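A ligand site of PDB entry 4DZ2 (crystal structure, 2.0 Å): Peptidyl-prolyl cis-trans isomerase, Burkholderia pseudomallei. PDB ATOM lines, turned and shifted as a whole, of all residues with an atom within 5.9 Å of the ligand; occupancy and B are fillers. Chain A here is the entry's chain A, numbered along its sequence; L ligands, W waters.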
ATOM      1  N   TYR A  33      -7.617  -1.390  -2.192  1.00  0.00           N
ATOM      2  CA  TYR A  33      -7.363  -1.609  -3.607  1.00  0.00           C
ATOM      3  C   TYR A  33      -7.392  -3.075  -3.956  1.00  0.00           C
ATOM      4  O   TYR A  33      -7.142  -3.952  -3.108  1.00  0.00           O
ATOM      5  CB  TYR A  33      -5.995  -1.005  -4.011  1.00  0.00           C
ATOM      6  CG  TYR A  33      -4.809  -1.755  -3.484  1.00  0.00           C
ATOM      7  CD1 TYR A  33      -4.212  -1.389  -2.274  1.00  0.00           C
ATOM      8  CD2 TYR A  33      -4.265  -2.854  -4.188  1.00  0.00           C
ATOM      9  CE1 TYR A  33      -3.117  -2.090  -1.763  1.00  0.00           C
ATOM     10  CE2 TYR A  33      -3.177  -3.567  -3.682  1.00  0.00           C
ATOM     11  CZ  TYR A  33      -2.591  -3.174  -2.461  1.00  0.00           C
ATOM     12  OH  TYR A  33      -1.505  -3.853  -1.931  1.00  0.00           O
ATOM     13  N   GLY A  35      -5.736  -5.353  -7.408  1.00  0.00           N
ATOM     14  CA  GLY A  35      -4.893  -5.230  -8.589  1.00  0.00           C
ATOM     15  C   GLY A  35      -5.013  -6.472  -9.456  1.00  0.00           C
ATOM     16  O   GLY A  35      -4.972  -7.604  -8.940  1.00  0.00           O
ATOM     17  N   PHE A  43      -3.635 -10.104  -8.562  1.00  0.00           N
ATOM     18  CA  PHE A  43      -2.310 -10.243  -7.905  1.00  0.00           C
ATOM     19  C   PHE A  43      -2.298  -9.713  -6.484  1.00  0.00           C
ATOM     20  O   PHE A  43      -1.419 -10.080  -5.720  1.00  0.00           O
ATOM     21  CB  PHE A  43      -1.151  -9.661  -8.737  1.00  0.00           C
ATOM     22  CG  PHE A  43      -1.323  -8.188  -9.100  1.00  0.00           C
ATOM     23  CD1 PHE A  43      -0.956  -7.179  -8.207  1.00  0.00           C
ATOM     24  CD2 PHE A  43      -1.800  -7.827 -10.336  1.00  0.00           C
ATOM     25  CE1 PHE A  43      -1.090  -5.851  -8.545  1.00  0.00           C
ATOM     26  CE2 PHE A  43      -1.945  -6.496 -10.666  1.00  0.00           C
ATOM     27  CZ  PHE A  43      -1.581  -5.504  -9.772  1.00  0.00           C
ATOM     28  N   ASP A  44      -3.266  -8.887  -6.119  1.00  0.00           N
ATOM     29  CA  ASP A  44      -3.320  -8.346  -4.738  1.00  0.00           C
ATOM     30  C   ASP A  44      -4.660  -7.739  -4.436  1.00  0.00           C
ATOM     31  O   ASP A  44      -5.399  -7.280  -5.343  1.00  0.00           O
ATOM     32  CB  ASP A  44      -2.211  -7.296  -4.531  1.00  0.00           C
ATOM     33  CG  ASP A  44      -1.904  -7.018  -3.042  1.00  0.00           C
ATOM     34  OD1 ASP A  44      -2.605  -7.486  -2.116  1.00  0.00           O
ATOM     35  OD2 ASP A  44      -0.921  -6.287  -2.820  1.00  0.00           O
ATOM     36  N   ARG A  49      -6.435  -9.021   2.774  1.00  0.00           N
ATOM     37  CA  ARG A  49      -5.494  -9.002   3.911  1.00  0.00           C
ATOM     38  C   ARG A  49      -6.046  -8.188   5.083  1.00  0.00           C
ATOM     39  O   ARG A  49      -5.404  -8.105   6.114  1.00  0.00           O
ATOM     40  CB  ARG A  49      -4.149  -8.405   3.473  1.00  0.00           C
ATOM     41  CG  ARG A  49      -3.532  -9.105   2.261  1.00  0.00           C
ATOM     42  CD  ARG A  49      -2.160  -8.538   1.933  1.00  0.00           C
ATOM     43  NE  ARG A  49      -2.200  -7.356   1.074  1.00  0.00           N
ATOM     44  CZ  ARG A  49      -2.103  -6.087   1.489  1.00  0.00           C
ATOM     45  NH1 ARG A  49      -1.950  -5.770   2.787  1.00  0.00           N
ATOM     46  NH2 ARG A  49      -2.142  -5.105   0.592  1.00  0.00           N
ATOM     47  N   PHE A  53      -4.425   0.487   2.965  1.00  0.00           N
ATOM     48  CA  PHE A  53      -3.111   0.947   2.562  1.00  0.00           C
ATOM     49  C   PHE A  53      -3.026   2.456   2.631  1.00  0.00           C
ATOM     50  O   PHE A  53      -3.812   3.160   2.008  1.00  0.00           O
ATOM     51  CB  PHE A  53      -2.803   0.446   1.147  1.00  0.00           C
ATOM     52  CG  PHE A  53      -1.507   0.951   0.589  1.00  0.00           C
ATOM     53  CD1 PHE A  53      -0.307   0.548   1.118  1.00  0.00           C
ATOM     54  CD2 PHE A  53      -1.515   1.840  -0.503  1.00  0.00           C
ATOM     55  CE1 PHE A  53       0.885   1.023   0.599  1.00  0.00           C
ATOM     56  CE2 PHE A  53      -0.329   2.303  -1.028  1.00  0.00           C
ATOM     57  CZ  PHE A  53       0.863   1.898  -0.484  1.00  0.00           C
ATOM     58  N   MET A  61       6.820   7.174  -3.833  1.00  0.00           N
ATOM     59  CA  MET A  61       7.095   5.871  -3.243  1.00  0.00           C
ATOM     60  C   MET A  61       6.297   4.746  -3.930  1.00  0.00           C
ATOM     61  O   MET A  61       6.711   3.566  -3.915  1.00  0.00           O
ATOM     62  CB  MET A  61       6.786   5.897  -1.756  1.00  0.00           C
ATOM     63  CG  MET A  61       7.610   6.940  -0.995  1.00  0.00           C
ATOM     64  SD  MET A  61       9.386   6.569  -1.004  1.00  0.00           S
ATOM     65  CE  MET A  61       9.423   5.077   0.005  1.00  0.00           C
ATOM     66  N   VAL A  62       5.177   5.101  -4.528  1.00  0.00           N
ATOM     67  CA  VAL A  62       4.325   4.129  -5.240  1.00  0.00           C
ATOM     68  C   VAL A  62       4.590   4.296  -6.715  1.00  0.00           C
ATOM     69  O   VAL A  62       5.205   5.221  -7.127  1.00  0.00           O
ATOM     70  CB  VAL A  62       2.824   4.327  -4.931  1.00  0.00           C
ATOM     71  CG1 VAL A  62       2.553   3.959  -3.464  1.00  0.00           C
ATOM     72  CG2 VAL A  62       2.375   5.753  -5.278  1.00  0.00           C
ATOM     73  N   ILE A  63       4.101   3.356  -7.517  1.00  0.00           N
ATOM     74  CA  ILE A  63       4.261   3.442  -8.974  1.00  0.00           C
ATOM     75  C   ILE A  63       3.640   4.719  -9.491  1.00  0.00           C
ATOM     76  O   ILE A  63       2.682   5.225  -8.912  1.00  0.00           O
ATOM     77  CB  ILE A  63       3.705   2.193  -9.702  1.00  0.00           C
ATOM     78  CG1 ILE A  63       2.231   1.933  -9.295  1.00  0.00           C
ATOM     79  CG2 ILE A  63       4.574   0.997  -9.396  1.00  0.00           C
ATOM     80  CD1 ILE A  63       1.622   0.698  -9.950  1.00  0.00           C
ATOM     81  N   TRP A  66      -0.234   5.407  -9.769  1.00  0.00           N
ATOM     82  CA  TRP A  66      -0.915   5.686  -8.524  1.00  0.00           C
ATOM     83  C   TRP A  66      -0.772   7.109  -8.047  1.00  0.00           C
ATOM     84  O   TRP A  66      -1.770   7.738  -7.689  1.00  0.00           O
ATOM     85  CB  TRP A  66      -0.430   4.752  -7.431  1.00  0.00           C
ATOM     86  CG  TRP A  66      -1.220   3.490  -7.307  1.00  0.00           C
ATOM     87  CD1 TRP A  66      -1.361   2.483  -8.248  1.00  0.00           C
ATOM     88  CD2 TRP A  66      -1.971   3.068  -6.155  1.00  0.00           C
ATOM     89  NE1 TRP A  66      -2.169   1.474  -7.743  1.00  0.00           N
ATOM     90  CE2 TRP A  66      -2.559   1.777  -6.482  1.00  0.00           C
ATOM     91  CE3 TRP A  66      -2.223   3.619  -4.901  1.00  0.00           C
ATOM     92  CZ2 TRP A  66      -3.363   1.073  -5.582  1.00  0.00           C
ATOM     93  CZ3 TRP A  66      -3.027   2.915  -4.001  1.00  0.00           C
ATOM     94  CH2 TRP A  66      -3.578   1.665  -4.328  1.00  0.00           C
ATOM     95  N   GLY A  88       4.058   1.735 -14.427  1.00  0.00           N
ATOM     96  CA  GLY A  88       3.978   0.651 -13.432  1.00  0.00           C
ATOM     97  C   GLY A  88       5.381   0.082 -13.163  1.00  0.00           C
ATOM     98  O   GLY A  88       6.243   0.801 -12.711  1.00  0.00           O
ATOM     99  N   TYR A  89       5.580  -1.198 -13.473  1.00  0.00           N
ATOM    100  CA  TYR A  89       6.866  -1.917 -13.191  1.00  0.00           C
ATOM    101  C   TYR A  89       7.750  -2.104 -14.425  1.00  0.00           C
ATOM    102  O   TYR A  89       8.794  -2.743 -14.355  1.00  0.00           O
ATOM    103  CB  TYR A  89       6.596  -3.259 -12.486  1.00  0.00           C
ATOM    104  CG  TYR A  89       5.940  -3.052 -11.132  1.00  0.00           C
ATOM    105  CD1 TYR A  89       6.716  -2.667 -10.029  1.00  0.00           C
ATOM    106  CD2 TYR A  89       4.572  -3.201 -10.969  1.00  0.00           C
ATOM    107  CE1 TYR A  89       6.130  -2.445  -8.774  1.00  0.00           C
ATOM    108  CE2 TYR A  89       3.971  -2.994  -9.719  1.00  0.00           C
ATOM    109  CZ  TYR A  89       4.756  -2.604  -8.616  1.00  0.00           C
ATOM    110  OH  TYR A  89       4.185  -2.366  -7.357  1.00  0.00           O
ATOM    111  N   GLY A  90       7.324  -1.541 -15.556  1.00  0.00           N
ATOM    112  CA  GLY A  90       8.105  -1.530 -16.775  1.00  0.00           C
ATOM    113  C   GLY A  90       8.608  -2.887 -17.263  1.00  0.00           C
ATOM    114  O   GLY A  90       7.945  -3.904 -17.050  1.00  0.00           O
ATOM    115  N   ALA A  94       7.630  -7.411 -11.408  1.00  0.00           N
ATOM    116  CA  ALA A  94       7.737  -7.420  -9.927  1.00  0.00           C
ATOM    117  C   ALA A  94       7.355  -8.750  -9.266  1.00  0.00           C
ATOM    118  O   ALA A  94       6.370  -9.404  -9.656  1.00  0.00           O
ATOM    119  CB  ALA A  94       6.923  -6.275  -9.342  1.00  0.00           C
ATOM    120  N   VAL A  97       5.318 -12.112  -9.971  1.00  0.00           N
ATOM    121  CA  VAL A  97       3.853 -12.160 -10.123  1.00  0.00           C
ATOM    122  C   VAL A  97       3.351 -11.149 -11.153  1.00  0.00           C
ATOM    123  O   VAL A  97       2.366 -11.409 -11.840  1.00  0.00           O
ATOM    124  CB  VAL A  97       3.122 -11.957  -8.764  1.00  0.00           C
ATOM    125  CG1 VAL A  97       3.571 -13.030  -7.779  1.00  0.00           C
ATOM    126  CG2 VAL A  97       3.364 -10.554  -8.190  1.00  0.00           C
ATOM    127  N   ILE A  98       4.037 -10.015 -11.268  1.00  0.00           N
ATOM    128  CA  ILE A  98       3.756  -9.059 -12.333  1.00  0.00           C
ATOM    129  C   ILE A  98       4.819  -9.214 -13.431  1.00  0.00           C
ATOM    130  O   ILE A  98       5.979  -8.903 -13.204  1.00  0.00           O
ATOM    131  CB  ILE A  98       3.712  -7.612 -11.834  1.00  0.00           C
ATOM    132  CG1 ILE A  98       2.488  -7.444 -10.914  1.00  0.00           C
ATOM    133  CG2 ILE A  98       3.636  -6.647 -13.012  1.00  0.00           C
ATOM    134  CD1 ILE A  98       2.422  -6.125 -10.182  1.00  0.00           C
ATOM    135  N   LEU A 104      -1.444  -2.738 -15.917  1.00  0.00           N
ATOM    136  CA  LEU A 104      -2.028  -3.105 -14.647  1.00  0.00           C
ATOM    137  C   LEU A 104      -3.395  -2.457 -14.499  1.00  0.00           C
ATOM    138  O   LEU A 104      -3.557  -1.287 -14.856  1.00  0.00           O
ATOM    139  CB  LEU A 104      -1.134  -2.648 -13.481  1.00  0.00           C
ATOM    140  CG  LEU A 104       0.330  -3.102 -13.447  1.00  0.00           C
ATOM    141  CD1 LEU A 104       1.045  -2.468 -12.245  1.00  0.00           C
ATOM    142  CD2 LEU A 104       0.489  -4.646 -13.467  1.00  0.00           C
ATOM    143  N   PHE A 106      -6.062  -1.465 -11.543  1.00  0.00           N
ATOM    144  CA  PHE A 106      -6.361  -1.364 -10.138  1.00  0.00           C
ATOM    145  C   PHE A 106      -7.752  -0.792  -9.929  1.00  0.00           C
ATOM    146  O   PHE A 106      -8.128   0.113 -10.609  1.00  0.00           O
ATOM    147  CB  PHE A 106      -5.348  -0.435  -9.451  1.00  0.00           C
ATOM    148  CG  PHE A 106      -3.996  -1.061  -9.186  1.00  0.00           C
ATOM    149  CD1 PHE A 106      -3.740  -1.725  -8.010  1.00  0.00           C
ATOM    150  CD2 PHE A 106      -2.972  -0.947 -10.104  1.00  0.00           C
ATOM    151  CE1 PHE A 106      -2.482  -2.272  -7.751  1.00  0.00           C
ATOM    152  CE2 PHE A 106      -1.725  -1.478  -9.868  1.00  0.00           C
ATOM    153  CZ  PHE A 106      -1.471  -2.135  -8.685  1.00  0.00           C
HETATM  154  C1  LIG L   1       2.993   0.118  -5.325  1.00  0.00           C
HETATM  155  C2  LIG L   1       1.674  -0.416  -5.806  1.00  0.00           C
HETATM  156  C3  LIG L   1       0.601   0.654  -5.625  1.00  0.00           C
HETATM  157  C4  LIG L   1       0.176   0.888  -4.188  1.00  0.00           C
HETATM  158  C5  LIG L   1      -0.351  -0.421  -3.630  1.00  0.00           C
HETATM  159  C6  LIG L   1       0.726  -1.482  -3.740  1.00  0.00           C
HETATM  160  C7  LIG L   1       1.190  -2.795  -5.847  1.00  0.00           C
HETATM  161  C8  LIG L   1       0.674  -4.036  -5.298  1.00  0.00           C
HETATM  162  C9  LIG L   1       1.617  -4.979  -4.588  1.00  0.00           C
HETATM  163  C10 LIG L   1       3.006  -5.045  -5.224  1.00  0.00           C
HETATM  164  C11 LIG L   1       4.062  -5.692  -4.267  1.00  0.00           C
HETATM  165  C12 LIG L   1       3.995  -5.114  -2.855  1.00  0.00           C
HETATM  166  C13 LIG L   1       2.537  -5.177  -2.370  1.00  0.00           C
HETATM  167  C14 LIG L   1       2.225  -4.624  -0.969  1.00  0.00           C
HETATM  168  C15 LIG L   1       2.796  -3.222  -0.713  1.00  0.00           C
HETATM  169  C16 LIG L   1       2.328  -2.595   0.615  1.00  0.00           C
HETATM  170  C17 LIG L   1       3.190  -3.025   1.824  1.00  0.00           C
HETATM  171  C18 LIG L   1       4.492  -2.239   1.864  1.00  0.00           C
HETATM  172  C19 LIG L   1       5.544  -2.849   1.286  1.00  0.00           C
HETATM  173  C20 LIG L   1       6.930  -2.335   1.136  1.00  0.00           C
HETATM  174  C21 LIG L   1       7.012  -1.686  -0.244  1.00  0.00           C
HETATM  175  C22 LIG L   1       6.731  -0.213  -0.399  1.00  0.00           C
HETATM  176  C23 LIG L   1       6.432   0.189  -1.845  1.00  0.00           C
HETATM  177  C24 LIG L   1       5.114  -0.369  -2.408  1.00  0.00           C
HETATM  178  C25 LIG L   1       4.946  -0.042  -3.886  1.00  0.00           C
HETATM  179  C26 LIG L   1       6.031  -0.675  -4.742  1.00  0.00           C
HETATM  180  C27 LIG L   1       6.841   0.165  -5.432  1.00  0.00           C
HETATM  181  C28 LIG L   1       7.975  -0.296  -6.307  1.00  0.00           C
HETATM  182  C29 LIG L   1       8.110   0.583  -7.549  1.00  0.00           C
HETATM  183  C30 LIG L   1       9.366   0.238  -8.347  1.00  0.00           C
HETATM  184  C31 LIG L   1      10.613   0.299  -7.462  1.00  0.00           C
HETATM  185  C32 LIG L   1      10.493  -0.564  -6.215  1.00  0.00           C
HETATM  186  C33 LIG L   1       9.230  -0.232  -5.437  1.00  0.00           C
HETATM  187  C34 LIG L   1       2.923  -5.738  -6.583  1.00  0.00           C
HETATM  188  C35 LIG L   1       0.852  -2.934   0.889  1.00  0.00           C
HETATM  189  C36 LIG L   1       4.554  -0.885   2.498  1.00  0.00           C
HETATM  190  C37 LIG L   1       7.854  -3.567   1.300  1.00  0.00           C
HETATM  191  C38 LIG L   1       9.193  -3.230   1.907  1.00  0.00           C
HETATM  192  C39 LIG L   1       9.953  -2.286   1.391  1.00  0.00           C
HETATM  193  C40 LIG L   1       3.905   0.120  -1.583  1.00  0.00           C
HETATM  194  C41 LIG L   1       6.186  -2.165  -4.763  1.00  0.00           C
HETATM  195  C42 LIG L   1       6.226  -5.403  -2.101  1.00  0.00           C
HETATM  196  C43 LIG L   1       1.676  -6.604   0.276  1.00  0.00           C
HETATM  197  C44 LIG L   1       8.980   0.502 -10.669  1.00  0.00           C
HETATM  198  N1  LIG L   1       1.181  -1.648  -5.130  1.00  0.00           N
HETATM  199  O1  LIG L   1       3.660  -0.550  -4.272  1.00  0.00           O
HETATM  200  O2  LIG L   1       3.476   1.136  -5.820  1.00  0.00           O
HETATM  201  O3  LIG L   1       1.607  -2.866  -6.984  1.00  0.00           O
HETATM  202  O4  LIG L   1      -0.513  -4.310  -5.421  1.00  0.00           O
HETATM  203  O5  LIG L   1       1.719  -4.434  -3.288  1.00  0.00           O
HETATM  204  O6  LIG L   1       1.075  -6.296  -4.549  1.00  0.00           O
HETATM  205  O7  LIG L   1       4.875  -5.832  -1.972  1.00  0.00           O
HETATM  206  O8  LIG L   1       2.656  -5.563   0.028  1.00  0.00           O
HETATM  207  O9  LIG L   1       7.273  -2.354  -1.233  1.00  0.00           O
HETATM  208  O10 LIG L   1       6.355   1.617  -1.878  1.00  0.00           O
HETATM  209  O11 LIG L   1       9.489   1.123  -9.475  1.00  0.00           O
HETATM  210  O12 LIG L   1      11.746  -0.171  -8.199  1.00  0.00           O
HETATM  211  O   HOH W   1       3.788  -1.172   5.691  1.00  0.00           O
HETATM  212  O   HOH W   2      13.819  -1.684  -7.177  1.00  0.00           O
HETATM  213  O   HOH W   3       5.193  -5.167   3.845  1.00  0.00           O
HETATM  214  O   HOH W   4      10.483  -3.146  -9.087  1.00  0.00           O
HETATM  215  O   HOH W   5       4.953  -6.362   1.176  1.00  0.00           O
HETATM  216  O   HOH W   6      10.774  -0.345 -13.195  1.00  0.00           O
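The backbone NH (N) of Ile 63 sits at hydrogen-bond distance from an oxygen (O2) of the ligand, at 2.9 Å.
The side-chain hydroxyl (OH) of Tyr 89 lies within hydrogen-bond range of an oxygen (O3) of the ligand (2.7 Å).
The side-chain carboxylate (OD2) of Asp 44 is in hydrogen-bond range of an oxygen (O6) of the ligand, at 2.6 Å.
O of Met 61 lies within hydrogen-bond range of O10 of the ligand.
OD2 of Asp 44 lies within hydrogen-bond range of OH of Tyr 33, 2.7 Å away.
The side-chain hydroxyl (OH) of Tyr 33 is in hydrogen-bond range of the guanidinium group (NH2) of Arg 49, 2.9 Å away.
The backbone carbonyl oxygen (O) of Gly 35 sits at hydrogen-bond distance from the backbone NH (N) of Phe 43, at 2.9 Å.
The side-chain carboxylate of Asp 44 lies within salt-bridge range of the guanidinium group of Arg 49 (3.2 Å).
The backbone NH (N) of Gly 35 sits at hydrogen-bond distance from the backbone carbonyl oxygen (O) of Asp 44.
Tyr 33 touches the ligand (CE2 to O4, 3.3 Å).
CE1 of Phe 43 touches O4 of the ligand, 3.5 Å away.
Arg 49 touches the ligand (NH2 to C35, 3.7 Å).
Phe 53 touches the ligand.
Val 62 touches the ligand (CA to O2, 3.2 Å).
Trp 66 touches the ligand.
Gly 88 touches the ligand (O to C44, 3.4 Å).
CD1 of Ile 98 touches C34 of the ligand, at 3.7 Å.
Phe 106 touches the ligand (CZ to O3, 3.6 Å).
Hydrophobic or aromatic side chains that line the ligand: Tyr 33, Phe 43, Phe 53, Val 62, Ile 63, Trp 66, Tyr 89, Ile 98 and Phe 106.
Of the 18 residues printed, 13 come within 4 Å of the ligand.
The nearest printed residue that does not touch the ligand is Ala 94 (4.9 Å).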
